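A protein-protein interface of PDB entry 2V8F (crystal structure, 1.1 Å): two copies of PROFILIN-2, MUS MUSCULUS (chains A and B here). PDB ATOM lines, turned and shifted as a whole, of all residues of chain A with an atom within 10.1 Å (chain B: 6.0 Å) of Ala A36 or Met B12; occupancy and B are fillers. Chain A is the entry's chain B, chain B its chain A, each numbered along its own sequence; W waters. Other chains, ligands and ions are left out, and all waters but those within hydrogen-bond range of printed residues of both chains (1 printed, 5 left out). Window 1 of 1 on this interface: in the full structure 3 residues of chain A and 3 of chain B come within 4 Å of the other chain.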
ATOM      1  N   GLN A   5     -19.434  18.797  -8.067  1.00  0.00           N
ATOM      2  CA  GLN A   5     -20.226  19.537  -9.038  1.00  0.00           C
ATOM      3  C   GLN A   5     -20.351  18.807 -10.357  1.00  0.00           C
ATOM      4  O   GLN A   5     -21.393  18.874 -11.043  1.00  0.00           O
ATOM      5  CB  GLN A   5     -19.645  20.941  -9.326  1.00  0.00           C
ATOM      6  CG  GLN A   5     -20.497  21.814 -10.231  1.00  0.00           C
ATOM      7  CD  GLN A   5     -21.881  22.119  -9.746  1.00  0.00           C
ATOM      8  OE1 GLN A   5     -22.900  22.065 -10.485  1.00  0.00           O
ATOM      9  NE2 GLN A   5     -21.960  22.518  -8.484  1.00  0.00           N
ATOM     10  N   VAL A   8     -23.304  16.509 -10.104  1.00  0.00           N
ATOM     11  CA  VAL A   8     -24.524  17.286 -10.280  1.00  0.00           C
ATOM     12  C   VAL A   8     -24.763  17.570 -11.759  1.00  0.00           C
ATOM     13  O   VAL A   8     -25.866  17.441 -12.314  1.00  0.00           O
ATOM     14  CB  VAL A   8     -24.515  18.552  -9.432  1.00  0.00           C
ATOM     15  CG1 VAL A   8     -25.659  19.503  -9.748  1.00  0.00           C
ATOM     16  CG2 VAL A   8     -24.453  18.179  -7.932  1.00  0.00           C
ATOM     17  N   ASP A   9     -23.712  18.012 -12.465  1.00  0.00           N
ATOM     18  CA  ASP A   9     -23.868  18.368 -13.875  1.00  0.00           C
ATOM     19  C   ASP A   9     -24.238  17.170 -14.724  1.00  0.00           C
ATOM     20  O   ASP A   9     -25.057  17.331 -15.637  1.00  0.00           O
ATOM     21  CB  ASP A   9     -22.539  18.978 -14.358  1.00  0.00           C
ATOM     22  CG  ASP A   9     -22.277  20.373 -13.864  1.00  0.00           C
ATOM     23  OD1 ASP A   9     -23.210  20.966 -13.273  1.00  0.00           O
ATOM     24  OD2 ASP A   9     -21.143  20.866 -14.053  1.00  0.00           O
ATOM     25  N   MET A  12     -27.904  16.635 -14.448  1.00  0.00           N
ATOM     26  CA  MET A  12     -28.709  17.693 -15.008  1.00  0.00           C
ATOM     27  C   MET A  12     -28.632  17.791 -16.537  1.00  0.00           C
ATOM     28  O   MET A  12     -29.410  18.503 -17.175  1.00  0.00           O
ATOM     29  CB  MET A  12     -28.212  19.002 -14.390  1.00  0.00           C
ATOM     30  CG  MET A  12     -28.606  19.206 -12.945  1.00  0.00           C
ATOM     31  SD  MET A  12     -30.364  19.379 -12.630  1.00  0.00           S
ATOM     32  CE  MET A  12     -30.588  21.076 -13.163  1.00  0.00           C
ATOM     33  N   GLN A  18     -34.875  19.729 -12.784  1.00  0.00           N
ATOM     34  CA  GLN A  18     -34.725  21.135 -12.409  1.00  0.00           C
ATOM     35  C   GLN A  18     -33.695  21.261 -11.282  1.00  0.00           C
ATOM     36  O   GLN A  18     -33.183  22.388 -11.131  1.00  0.00           O
ATOM     37  CB  GLN A  18     -35.974  21.824 -11.952  1.00  0.00           C
ATOM     38  CG  GLN A  18     -36.575  21.091 -10.758  1.00  0.00           C
ATOM     39  CD  GLN A  18     -37.809  21.862 -10.306  1.00  0.00           C
ATOM     40  OE1 GLN A  18     -37.660  22.971  -9.776  1.00  0.00           O
ATOM     41  NE2 GLN A  18     -38.979  21.305 -10.512  1.00  0.00           N
ATOM     42  N   GLU A  19     -33.319  20.220 -10.560  1.00  0.00           N
ATOM     43  CA  GLU A  19     -32.186  20.293  -9.630  1.00  0.00           C
ATOM     44  C   GLU A  19     -31.674  18.891  -9.311  1.00  0.00           C
ATOM     45  O   GLU A  19     -32.370  17.887  -9.556  1.00  0.00           O
ATOM     46  CB  GLU A  19     -32.466  21.059  -8.396  1.00  0.00           C
ATOM     47  CG  GLU A  19     -33.752  21.041  -7.701  1.00  0.00           C
ATOM     48  CD  GLU A  19     -33.771  21.802  -6.390  1.00  0.00           C
ATOM     49  OE1 GLU A  19     -32.856  21.513  -5.597  1.00  0.00           O
ATOM     50  OE2 GLU A  19     -34.694  22.606  -6.133  1.00  0.00           O
ATOM     51  N   ALA A  20     -30.466  18.834  -8.757  1.00  0.00           N
ATOM     52  CA  ALA A  20     -29.802  17.611  -8.396  1.00  0.00           C
ATOM     53  C   ALA A  20     -28.847  17.866  -7.247  1.00  0.00           C
ATOM     54  O   ALA A  20     -28.432  19.010  -7.052  1.00  0.00           O
ATOM     55  CB  ALA A  20     -29.116  16.967  -9.600  1.00  0.00           C
ATOM     56  N   ALA A  21     -28.507  16.823  -6.526  1.00  0.00           N
ATOM     57  CA  ALA A  21     -27.631  16.963  -5.407  1.00  0.00           C
ATOM     58  C   ALA A  21     -26.916  15.653  -5.108  1.00  0.00           C
ATOM     59  O   ALA A  21     -27.455  14.562  -5.300  1.00  0.00           O
ATOM     60  CB  ALA A  21     -28.315  17.500  -4.156  1.00  0.00           C
ATOM     61  N   VAL A  31     -25.106  18.114   2.695  1.00  0.00           N
ATOM     62  CA  VAL A  31     -25.040  18.269   1.251  1.00  0.00           C
ATOM     63  C   VAL A  31     -23.605  18.555   0.798  1.00  0.00           C
ATOM     64  O   VAL A  31     -22.937  19.444   1.310  1.00  0.00           O
ATOM     65  CB  VAL A  31     -25.939  19.428   0.821  1.00  0.00           C
ATOM     66  CG1 VAL A  31     -25.814  19.671  -0.684  1.00  0.00           C
ATOM     67  CG2 VAL A  31     -27.390  19.157   1.256  1.00  0.00           C
ATOM     68  N   ALA A  33     -22.785  18.732  -2.842  1.00  0.00           N
ATOM     69  CA  ALA A  33     -22.960  19.568  -3.998  1.00  0.00           C
ATOM     70  C   ALA A  33     -24.431  19.580  -4.392  1.00  0.00           C
ATOM     71  O   ALA A  33     -25.120  18.552  -4.235  1.00  0.00           O
ATOM     72  CB  ALA A  33     -22.174  19.042  -5.199  1.00  0.00           C
ATOM     73  N   ALA A  34     -24.940  20.697  -4.866  1.00  0.00           N
ATOM     74  CA  ALA A  34     -26.328  20.783  -5.261  1.00  0.00           C
ATOM     75  C   ALA A  34     -26.532  21.986  -6.187  1.00  0.00           C
ATOM     76  O   ALA A  34     -25.805  22.980  -6.089  1.00  0.00           O
ATOM     77  CB  ALA A  34     -27.228  20.997  -4.036  1.00  0.00           C
ATOM     78  N   THR A  35     -27.543  21.900  -7.020  1.00  0.00           N
ATOM     79  CA  THR A  35     -27.970  23.030  -7.832  1.00  0.00           C
ATOM     80  C   THR A  35     -28.130  24.255  -6.943  1.00  0.00           C
ATOM     81  O   THR A  35     -28.787  24.200  -5.926  1.00  0.00           O
ATOM     82  CB  THR A  35     -29.307  22.685  -8.485  1.00  0.00           C
ATOM     83  OG1 THR A  35     -29.172  21.490  -9.253  1.00  0.00           O
ATOM     84  CG2 THR A  35     -29.816  23.806  -9.364  1.00  0.00           C
ATOM     85  N   ALA A  36     -27.502  25.372  -7.287  1.00  0.00           N
ATOM     86  CA  ALA A  36     -27.498  26.529  -6.447  1.00  0.00           C
ATOM     87  C   ALA A  36     -28.895  27.124  -6.350  1.00  0.00           C
ATOM     88  O   ALA A  36     -29.611  27.240  -7.344  1.00  0.00           O
ATOM     89  CB  ALA A  36     -26.532  27.570  -6.978  1.00  0.00           C
ATOM     90  N   GLY A  37     -29.269  27.507  -5.142  1.00  0.00           N
ATOM     91  CA  GLY A  37     -30.451  28.253  -4.814  1.00  0.00           C
ATOM     92  C   GLY A  37     -31.724  27.439  -4.872  1.00  0.00           C
ATOM     93  O   GLY A  37     -32.802  28.002  -4.801  1.00  0.00           O
ATOM     94  N   GLY A  38     -31.603  26.109  -4.973  1.00  0.00           N
ATOM     95  CA  GLY A  38     -32.794  25.277  -4.950  1.00  0.00           C
ATOM     96  C   GLY A  38     -33.138  24.682  -3.609  1.00  0.00           C
ATOM     97  O   GLY A  38     -32.619  25.046  -2.547  1.00  0.00           O
ATOM     98  N   VAL A  39     -34.036  23.706  -3.605  1.00  0.00           N
ATOM     99  CA  VAL A  39     -34.495  23.029  -2.433  1.00  0.00           C
ATOM    100  C   VAL A  39     -33.445  22.097  -1.884  1.00  0.00           C
ATOM    101  O   VAL A  39     -33.205  22.034  -0.671  1.00  0.00           O
ATOM    102  CB  VAL A  39     -35.764  22.214  -2.815  1.00  0.00           C
ATOM    103  CG1 VAL A  39     -36.172  21.313  -1.681  1.00  0.00           C
ATOM    104  CG2 VAL A  39     -36.881  23.164  -3.206  1.00  0.00           C
ATOM    105  N   PHE A  40     -32.809  21.313  -2.766  1.00  0.00           N
ATOM    106  CA  PHE A  40     -31.896  20.318  -2.249  1.00  0.00           C
ATOM    107  C   PHE A  40     -30.688  20.875  -1.481  1.00  0.00           C
ATOM    108  O   PHE A  40     -30.172  20.263  -0.547  1.00  0.00           O
ATOM    109  CB  PHE A  40     -31.347  19.406  -3.337  1.00  0.00           C
ATOM    110  CG  PHE A  40     -32.374  18.517  -4.023  1.00  0.00           C
ATOM    111  CD1 PHE A  40     -33.525  18.079  -3.421  1.00  0.00           C
ATOM    112  CD2 PHE A  40     -32.129  18.119  -5.330  1.00  0.00           C
ATOM    113  CE1 PHE A  40     -34.404  17.209  -4.072  1.00  0.00           C
ATOM    114  CE2 PHE A  40     -32.954  17.217  -5.983  1.00  0.00           C
ATOM    115  CZ  PHE A  40     -34.090  16.793  -5.336  1.00  0.00           C
ATOM    116  N   GLN A  41     -30.229  22.070  -1.913  1.00  0.00           N
ATOM    117  CA  GLN A  41     -29.086  22.678  -1.225  1.00  0.00           C
ATOM    118  C   GLN A  41     -29.393  22.920   0.250  1.00  0.00           C
ATOM    119  O   GLN A  41     -28.454  23.013   1.053  1.00  0.00           O
ATOM    120  CB  GLN A  41     -28.836  24.035  -1.888  1.00  0.00           C
ATOM    121  CG  GLN A  41     -27.670  24.850  -1.364  1.00  0.00           C
ATOM    122  CD  GLN A  41     -27.435  26.108  -2.176  1.00  0.00           C
ATOM    123  OE1 GLN A  41     -28.271  26.690  -2.856  1.00  0.00           O
ATOM    124  NE2 GLN A  41     -26.183  26.559  -2.108  1.00  0.00           N
ATOM    125  N   SER A  42     -30.684  23.029   0.583  1.00  0.00           N
ATOM    126  CA  SER A  42     -31.169  23.282   1.923  1.00  0.00           C
ATOM    127  C   SER A  42     -31.512  22.022   2.725  1.00  0.00           C
ATOM    128  O   SER A  42     -31.969  22.102   3.852  1.00  0.00           O
ATOM    129  CB  SER A  42     -32.406  24.178   1.906  1.00  0.00           C
ATOM    130  OG  SER A  42     -32.035  25.505   1.572  1.00  0.00           O
ATOM    131  N   TYR B   7     -18.285  29.382  -3.503  1.00  0.00           N
ATOM    132  CA  TYR B   7     -18.645  30.723  -3.001  1.00  0.00           C
ATOM    133  C   TYR B   7     -19.904  31.244  -3.656  1.00  0.00           C
ATOM    134  O   TYR B   7     -20.732  31.873  -2.989  1.00  0.00           O
ATOM    135  CB  TYR B   7     -17.459  31.681  -3.230  1.00  0.00           C
ATOM    136  CG  TYR B   7     -16.400  31.415  -2.168  1.00  0.00           C
ATOM    137  CD1 TYR B   7     -16.269  32.327  -1.140  1.00  0.00           C
ATOM    138  CD2 TYR B   7     -15.543  30.294  -2.191  1.00  0.00           C
ATOM    139  CE1 TYR B   7     -15.335  32.176  -0.138  1.00  0.00           C
ATOM    140  CE2 TYR B   7     -14.603  30.138  -1.166  1.00  0.00           C
ATOM    141  CZ  TYR B   7     -14.506  31.062  -0.161  1.00  0.00           C
ATOM    142  OH  TYR B   7     -13.602  30.924   0.846  1.00  0.00           O
ATOM    143  N   VAL B   8     -20.043  30.996  -4.948  1.00  0.00           N
ATOM    144  CA  VAL B   8     -21.319  31.295  -5.605  1.00  0.00           C
ATOM    145  C   VAL B   8     -22.447  30.544  -4.942  1.00  0.00           C
ATOM    146  O   VAL B   8     -23.509  31.147  -4.696  1.00  0.00           O
ATOM    147  CB  VAL B   8     -21.200  31.006  -7.115  1.00  0.00           C
ATOM    148  CG1 VAL B   8     -22.516  31.180  -7.857  1.00  0.00           C
ATOM    149  CG2 VAL B   8     -20.197  31.895  -7.835  1.00  0.00           C
ATOM    150  N   ASP B   9     -22.234  29.259  -4.696  1.00  0.00           N
ATOM    151  CA  ASP B   9     -23.276  28.452  -4.023  1.00  0.00           C
ATOM    152  C   ASP B   9     -23.720  29.102  -2.713  1.00  0.00           C
ATOM    153  O   ASP B   9     -24.892  29.174  -2.391  1.00  0.00           O
ATOM    154  CB  ASP B   9     -22.719  27.064  -3.774  1.00  0.00           C
ATOM    155  CG  ASP B   9     -22.540  26.166  -4.943  1.00  0.00           C
ATOM    156  OD1 ASP B   9     -23.002  26.561  -6.025  1.00  0.00           O
ATOM    157  OD2 ASP B   9     -21.933  25.059  -4.845  1.00  0.00           O
ATOM    158  N   ASN B  10     -22.749  29.524  -1.924  1.00  0.00           N
ATOM    159  CA  ASN B  10     -23.003  30.097  -0.615  1.00  0.00           C
ATOM    160  C   ASN B  10     -23.837  31.361  -0.772  1.00  0.00           C
ATOM    161  O   ASN B  10     -24.814  31.582  -0.072  1.00  0.00           O
ATOM    162  CB  ASN B  10     -21.650  30.310   0.063  1.00  0.00           C
ATOM    163  CG  ASN B  10     -21.831  31.046   1.362  1.00  0.00           C
ATOM    164  OD1 ASN B  10     -22.135  32.246   1.435  1.00  0.00           O
ATOM    165  ND2 ASN B  10     -21.653  30.294   2.431  1.00  0.00           N
ATOM    166  N   LEU B  11     -23.471  32.182  -1.750  1.00  0.00           N
ATOM    167  CA  LEU B  11     -24.181  33.460  -1.937  1.00  0.00           C
ATOM    168  C   LEU B  11     -25.602  33.241  -2.425  1.00  0.00           C
ATOM    169  O   LEU B  11     -26.459  34.106  -2.255  1.00  0.00           O
ATOM    170  CB  LEU B  11     -23.405  34.312  -2.930  1.00  0.00           C
ATOM    171  CG  LEU B  11     -22.065  34.877  -2.426  1.00  0.00           C
ATOM    172  CD1 LEU B  11     -21.184  35.328  -3.577  1.00  0.00           C
ATOM    173  CD2 LEU B  11     -22.282  35.981  -1.415  1.00  0.00           C
ATOM    174  N   MET B  12     -25.846  32.125  -3.094  1.00  0.00           N
ATOM    175  CA  MET B  12     -27.164  31.774  -3.611  1.00  0.00           C
ATOM    176  C   MET B  12     -28.026  30.988  -2.618  1.00  0.00           C
ATOM    177  O   MET B  12     -29.196  30.770  -2.898  1.00  0.00           O
ATOM    178  CB  MET B  12     -27.023  30.936  -4.876  1.00  0.00           C
ATOM    179  CG  MET B  12     -26.431  31.709  -6.036  1.00  0.00           C
ATOM    180  SD  MET B  12     -27.536  32.942  -6.712  1.00  0.00           S
ATOM    181  CE  MET B  12     -28.627  31.839  -7.639  1.00  0.00           C
ATOM    182  N   CYS B  13     -27.457  30.515  -1.524  1.00  0.00           N
ATOM    183  CA  CYS B  13     -28.203  29.511  -0.770  1.00  0.00           C
ATOM    184  C   CYS B  13     -29.471  30.032  -0.125  1.00  0.00           C
ATOM    185  O   CYS B  13     -30.352  29.194   0.100  1.00  0.00           O
ATOM    186  CB  CYS B  13     -27.253  28.986   0.317  1.00  0.00           C
ATOM    187  SG  CYS B  13     -28.012  27.587   1.171  1.00  0.00           S
ATOM    188  N   ASP B  14     -29.564  31.328   0.164  1.00  0.00           N
ATOM    189  CA  ASP B  14     -30.737  31.778   0.931  1.00  0.00           C
ATOM    190  C   ASP B  14     -31.961  32.008   0.056  1.00  0.00           C
ATOM    191  O   ASP B  14     -33.020  32.416   0.547  1.00  0.00           O
ATOM    192  CB  ASP B  14     -30.360  33.025   1.744  1.00  0.00           C
ATOM    193  CG  ASP B  14     -30.021  34.268   0.972  1.00  0.00           C
ATOM    194  OD1 ASP B  14     -30.325  34.332  -0.239  1.00  0.00           O
ATOM    195  OD2 ASP B  14     -29.442  35.224   1.573  1.00  0.00           O
ATOM    196  N   GLY B  15     -31.854  31.776  -1.242  1.00  0.00           N
ATOM    197  CA  GLY B  15     -32.933  31.945  -2.177  1.00  0.00           C
ATOM    198  C   GLY B  15     -33.251  33.386  -2.514  1.00  0.00           C
ATOM    199  O   GLY B  15     -34.221  33.627  -3.250  1.00  0.00           O
ATOM    200  N   CYS B  16     -32.481  34.374  -2.021  1.00  0.00           N
ATOM    201  CA  CYS B  16     -32.869  35.756  -2.348  1.00  0.00           C
ATOM    202  C   CYS B  16     -32.130  36.320  -3.548  1.00  0.00           C
ATOM    203  O   CYS B  16     -32.479  37.408  -3.980  1.00  0.00           O
ATOM    204  CB  CYS B  16     -32.724  36.659  -1.127  1.00  0.00           C
ATOM    205  SG  CYS B  16     -31.110  37.356  -0.768  1.00  0.00           S
ATOM    206  N   CSX B  17     -31.171  35.569  -4.069  1.00  0.00           N
ATOM    207  CA  CSX B  17     -30.344  36.057  -5.193  1.00  0.00           C
ATOM    208  CB  CSX B  17     -28.843  35.913  -4.877  1.00  0.00           C
ATOM    209  SG  CSX B  17     -28.308  37.092  -3.602  1.00  0.00           S
ATOM    210  C   CSX B  17     -30.649  35.302  -6.482  1.00  0.00           C
ATOM    211  O   CSX B  17     -30.817  34.065  -6.499  1.00  0.00           O
ATOM    212  OD  CSX B  17     -28.804  36.398  -2.363  1.00  0.00           O
ATOM    213  N   GLN B  18     -30.678  36.079  -7.562  1.00  0.00           N
ATOM    214  CA  GLN B  18     -30.836  35.593  -8.916  1.00  0.00           C
ATOM    215  C   GLN B  18     -29.512  35.128  -9.506  1.00  0.00           C
ATOM    216  O   GLN B  18     -29.471  34.200 -10.301  1.00  0.00           O
ATOM    217  CB  GLN B  18     -31.199  36.921  -9.646  1.00  0.00           C
ATOM    218  CG  GLN B  18     -31.513  36.748 -11.115  1.00  0.00           C
ATOM    219  CD  GLN B  18     -32.791  35.962 -11.342  1.00  0.00           C
ATOM    220  OE1 GLN B  18     -33.638  35.917 -10.450  1.00  0.00           O
ATOM    221  NE2 GLN B  18     -32.922  35.354 -12.512  1.00  0.00           N
ATOM    222  N   GLU B  19     -28.417  35.747  -9.107  1.00  0.00           N
ATOM    223  CA  GLU B  19     -27.078  35.348  -9.512  1.00  0.00           C
ATOM    224  C   GLU B  19     -26.025  35.893  -8.552  1.00  0.00           C
ATOM    225  O   GLU B  19     -26.306  36.812  -7.775  1.00  0.00           O
ATOM    226  CB  GLU B  19     -26.804  35.700 -10.962  1.00  0.00           C
ATOM    227  CG  GLU B  19     -27.098  37.080 -11.432  1.00  0.00           C
ATOM    228  CD  GLU B  19     -26.673  37.331 -12.852  1.00  0.00           C
ATOM    229  OE1 GLU B  19     -25.497  37.006 -13.139  1.00  0.00           O
ATOM    230  OE2 GLU B  19     -27.419  37.799 -13.704  1.00  0.00           O
ATOM    231  N   ALA B  20     -24.853  35.304  -8.626  1.00  0.00           N
ATOM    232  CA  ALA B  20     -23.707  35.719  -7.808  1.00  0.00           C
ATOM    233  C   ALA B  20     -22.440  35.443  -8.587  1.00  0.00           C
ATOM    234  O   ALA B  20     -22.419  34.639  -9.511  1.00  0.00           O
ATOM    235  CB  ALA B  20     -23.656  35.081  -6.434  1.00  0.00           C
ATOM    236  N   THR B  35     -22.775  32.447 -11.522  1.00  0.00           N
ATOM    237  CA  THR B  35     -24.017  31.794 -11.935  1.00  0.00           C
ATOM    238  C   THR B  35     -24.089  31.692 -13.441  1.00  0.00           C
ATOM    239  O   THR B  35     -23.844  32.662 -14.122  1.00  0.00           O
ATOM    240  CB  THR B  35     -25.185  32.669 -11.424  1.00  0.00           C
ATOM    241  OG1 THR B  35     -25.135  32.730 -10.001  1.00  0.00           O
ATOM    242  CG2 THR B  35     -26.549  32.110 -11.865  1.00  0.00           C
ATOM    243  N   MET B 114     -26.831  39.662  -7.143  1.00  0.00           N
ATOM    244  CA  MET B 114     -28.028  40.256  -7.681  1.00  0.00           C
ATOM    245  C   MET B 114     -29.257  39.669  -7.012  1.00  0.00           C
ATOM    246  O   MET B 114     -29.422  38.461  -6.988  1.00  0.00           O
ATOM    247  CB  MET B 114     -28.098  40.038  -9.203  1.00  0.00           C
ATOM    248  CG  MET B 114     -29.317  40.727  -9.802  1.00  0.00           C
ATOM    249  SD  MET B 114     -29.547  40.357 -11.535  1.00  0.00           S
ATOM    250  CE  MET B 114     -28.071  40.977 -12.301  1.00  0.00           C
ATOM    251  N   LYS B 127     -24.770  40.855   2.668  1.00  0.00           N
ATOM    252  CA  LYS B 127     -24.195  39.644   2.093  1.00  0.00           C
ATOM    253  C   LYS B 127     -22.856  39.880   1.419  1.00  0.00           C
ATOM    254  O   LYS B 127     -21.887  39.175   1.652  1.00  0.00           O
ATOM    255  CB  LYS B 127     -25.193  39.110   1.063  1.00  0.00           C
ATOM    256  CG  LYS B 127     -24.874  37.768   0.441  1.00  0.00           C
ATOM    257  CD  LYS B 127     -26.029  37.207  -0.378  1.00  0.00           C
ATOM    258  CE  LYS B 127     -27.164  36.721   0.510  1.00  0.00           C
ATOM    259  NZ  LYS B 127     -26.859  35.424   1.188  1.00  0.00           N
HETATM  260  O   HOH W   1     -23.811  24.338  -7.530  1.00  0.00           O
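The side-chain sulfur (SD) of Met B12 sits close to the backbone NH (N) of Glu B19. The side-chain amide oxygen (OE1) of Gln A41 sits at hydrogen-bond distance from the backbone NH (N) of Gly A37.
O of Asp B9 sits at hydrogen-bond distance from NE2 of Gln A41 (2.9 Å).
Among the printed residues, merely in contact across the chains: Ala A36 with Asp B9, Ala A36 with Met B12, Gly A37 with Met B12 and Gln A41 with Cys B13.
Of the 19 printed residues of chain A, 3 touch a printed residue of chain B. Printed residues of chain B that touch a printed residue of chain A: Asp B9, Met B12 and Cys B13. Hydrophobic or aromatic side chains of chain B that line the printed part of chain A: Met B12. Among the printed residues, 5 pairs touch across the chains.
Water W1 lies within hydrogen-bond range of the side-chain amide nitrogen of Gln A5 (2.8 Å), the side-chain carboxylate of Asp B9 (2.8 Å) and the backbone carbonyl oxygen of Ala A34 (2.8 Å).
Positions printed for both chains: 8, 9, 12, 18, 19, 20 and 35. Of the 5 pairs that touch across the chains among the printed residues, none has its exchanged pair printed and touching as well.
Of the printed residues of chain B, Ala A36 touches Asp B9 (3.8 Å) and Met B12 (3.999 Å). Printed residues of chain A within 4 Å of Met B12: Ala A36 and Gly A37. No residue of chain A comes within 4 Å of Leu B11. Of the printed residues of chain A, Asp B9 touches Ala A36 (3.8 Å) and Gln A41 (2.9 Å). Of the printed residues of chain A, Cys B13 touches Gln A41. Printed residues of chain B within 4 Å of Gln A41: Asp B9 and Cys B13. Of the printed residues of chain B, Gly A37 touches Met B12. Ala A21 touches none of the printed residues of chain B. Ala A33 touches none of the printed residues of chain B. The nearest printed residue of chain B that does not touch Ala A36 is Val B8 (5.2 Å). The nearest printed residue of chain A that does not touch Met B12 is Gln A41 (4.2 Å).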
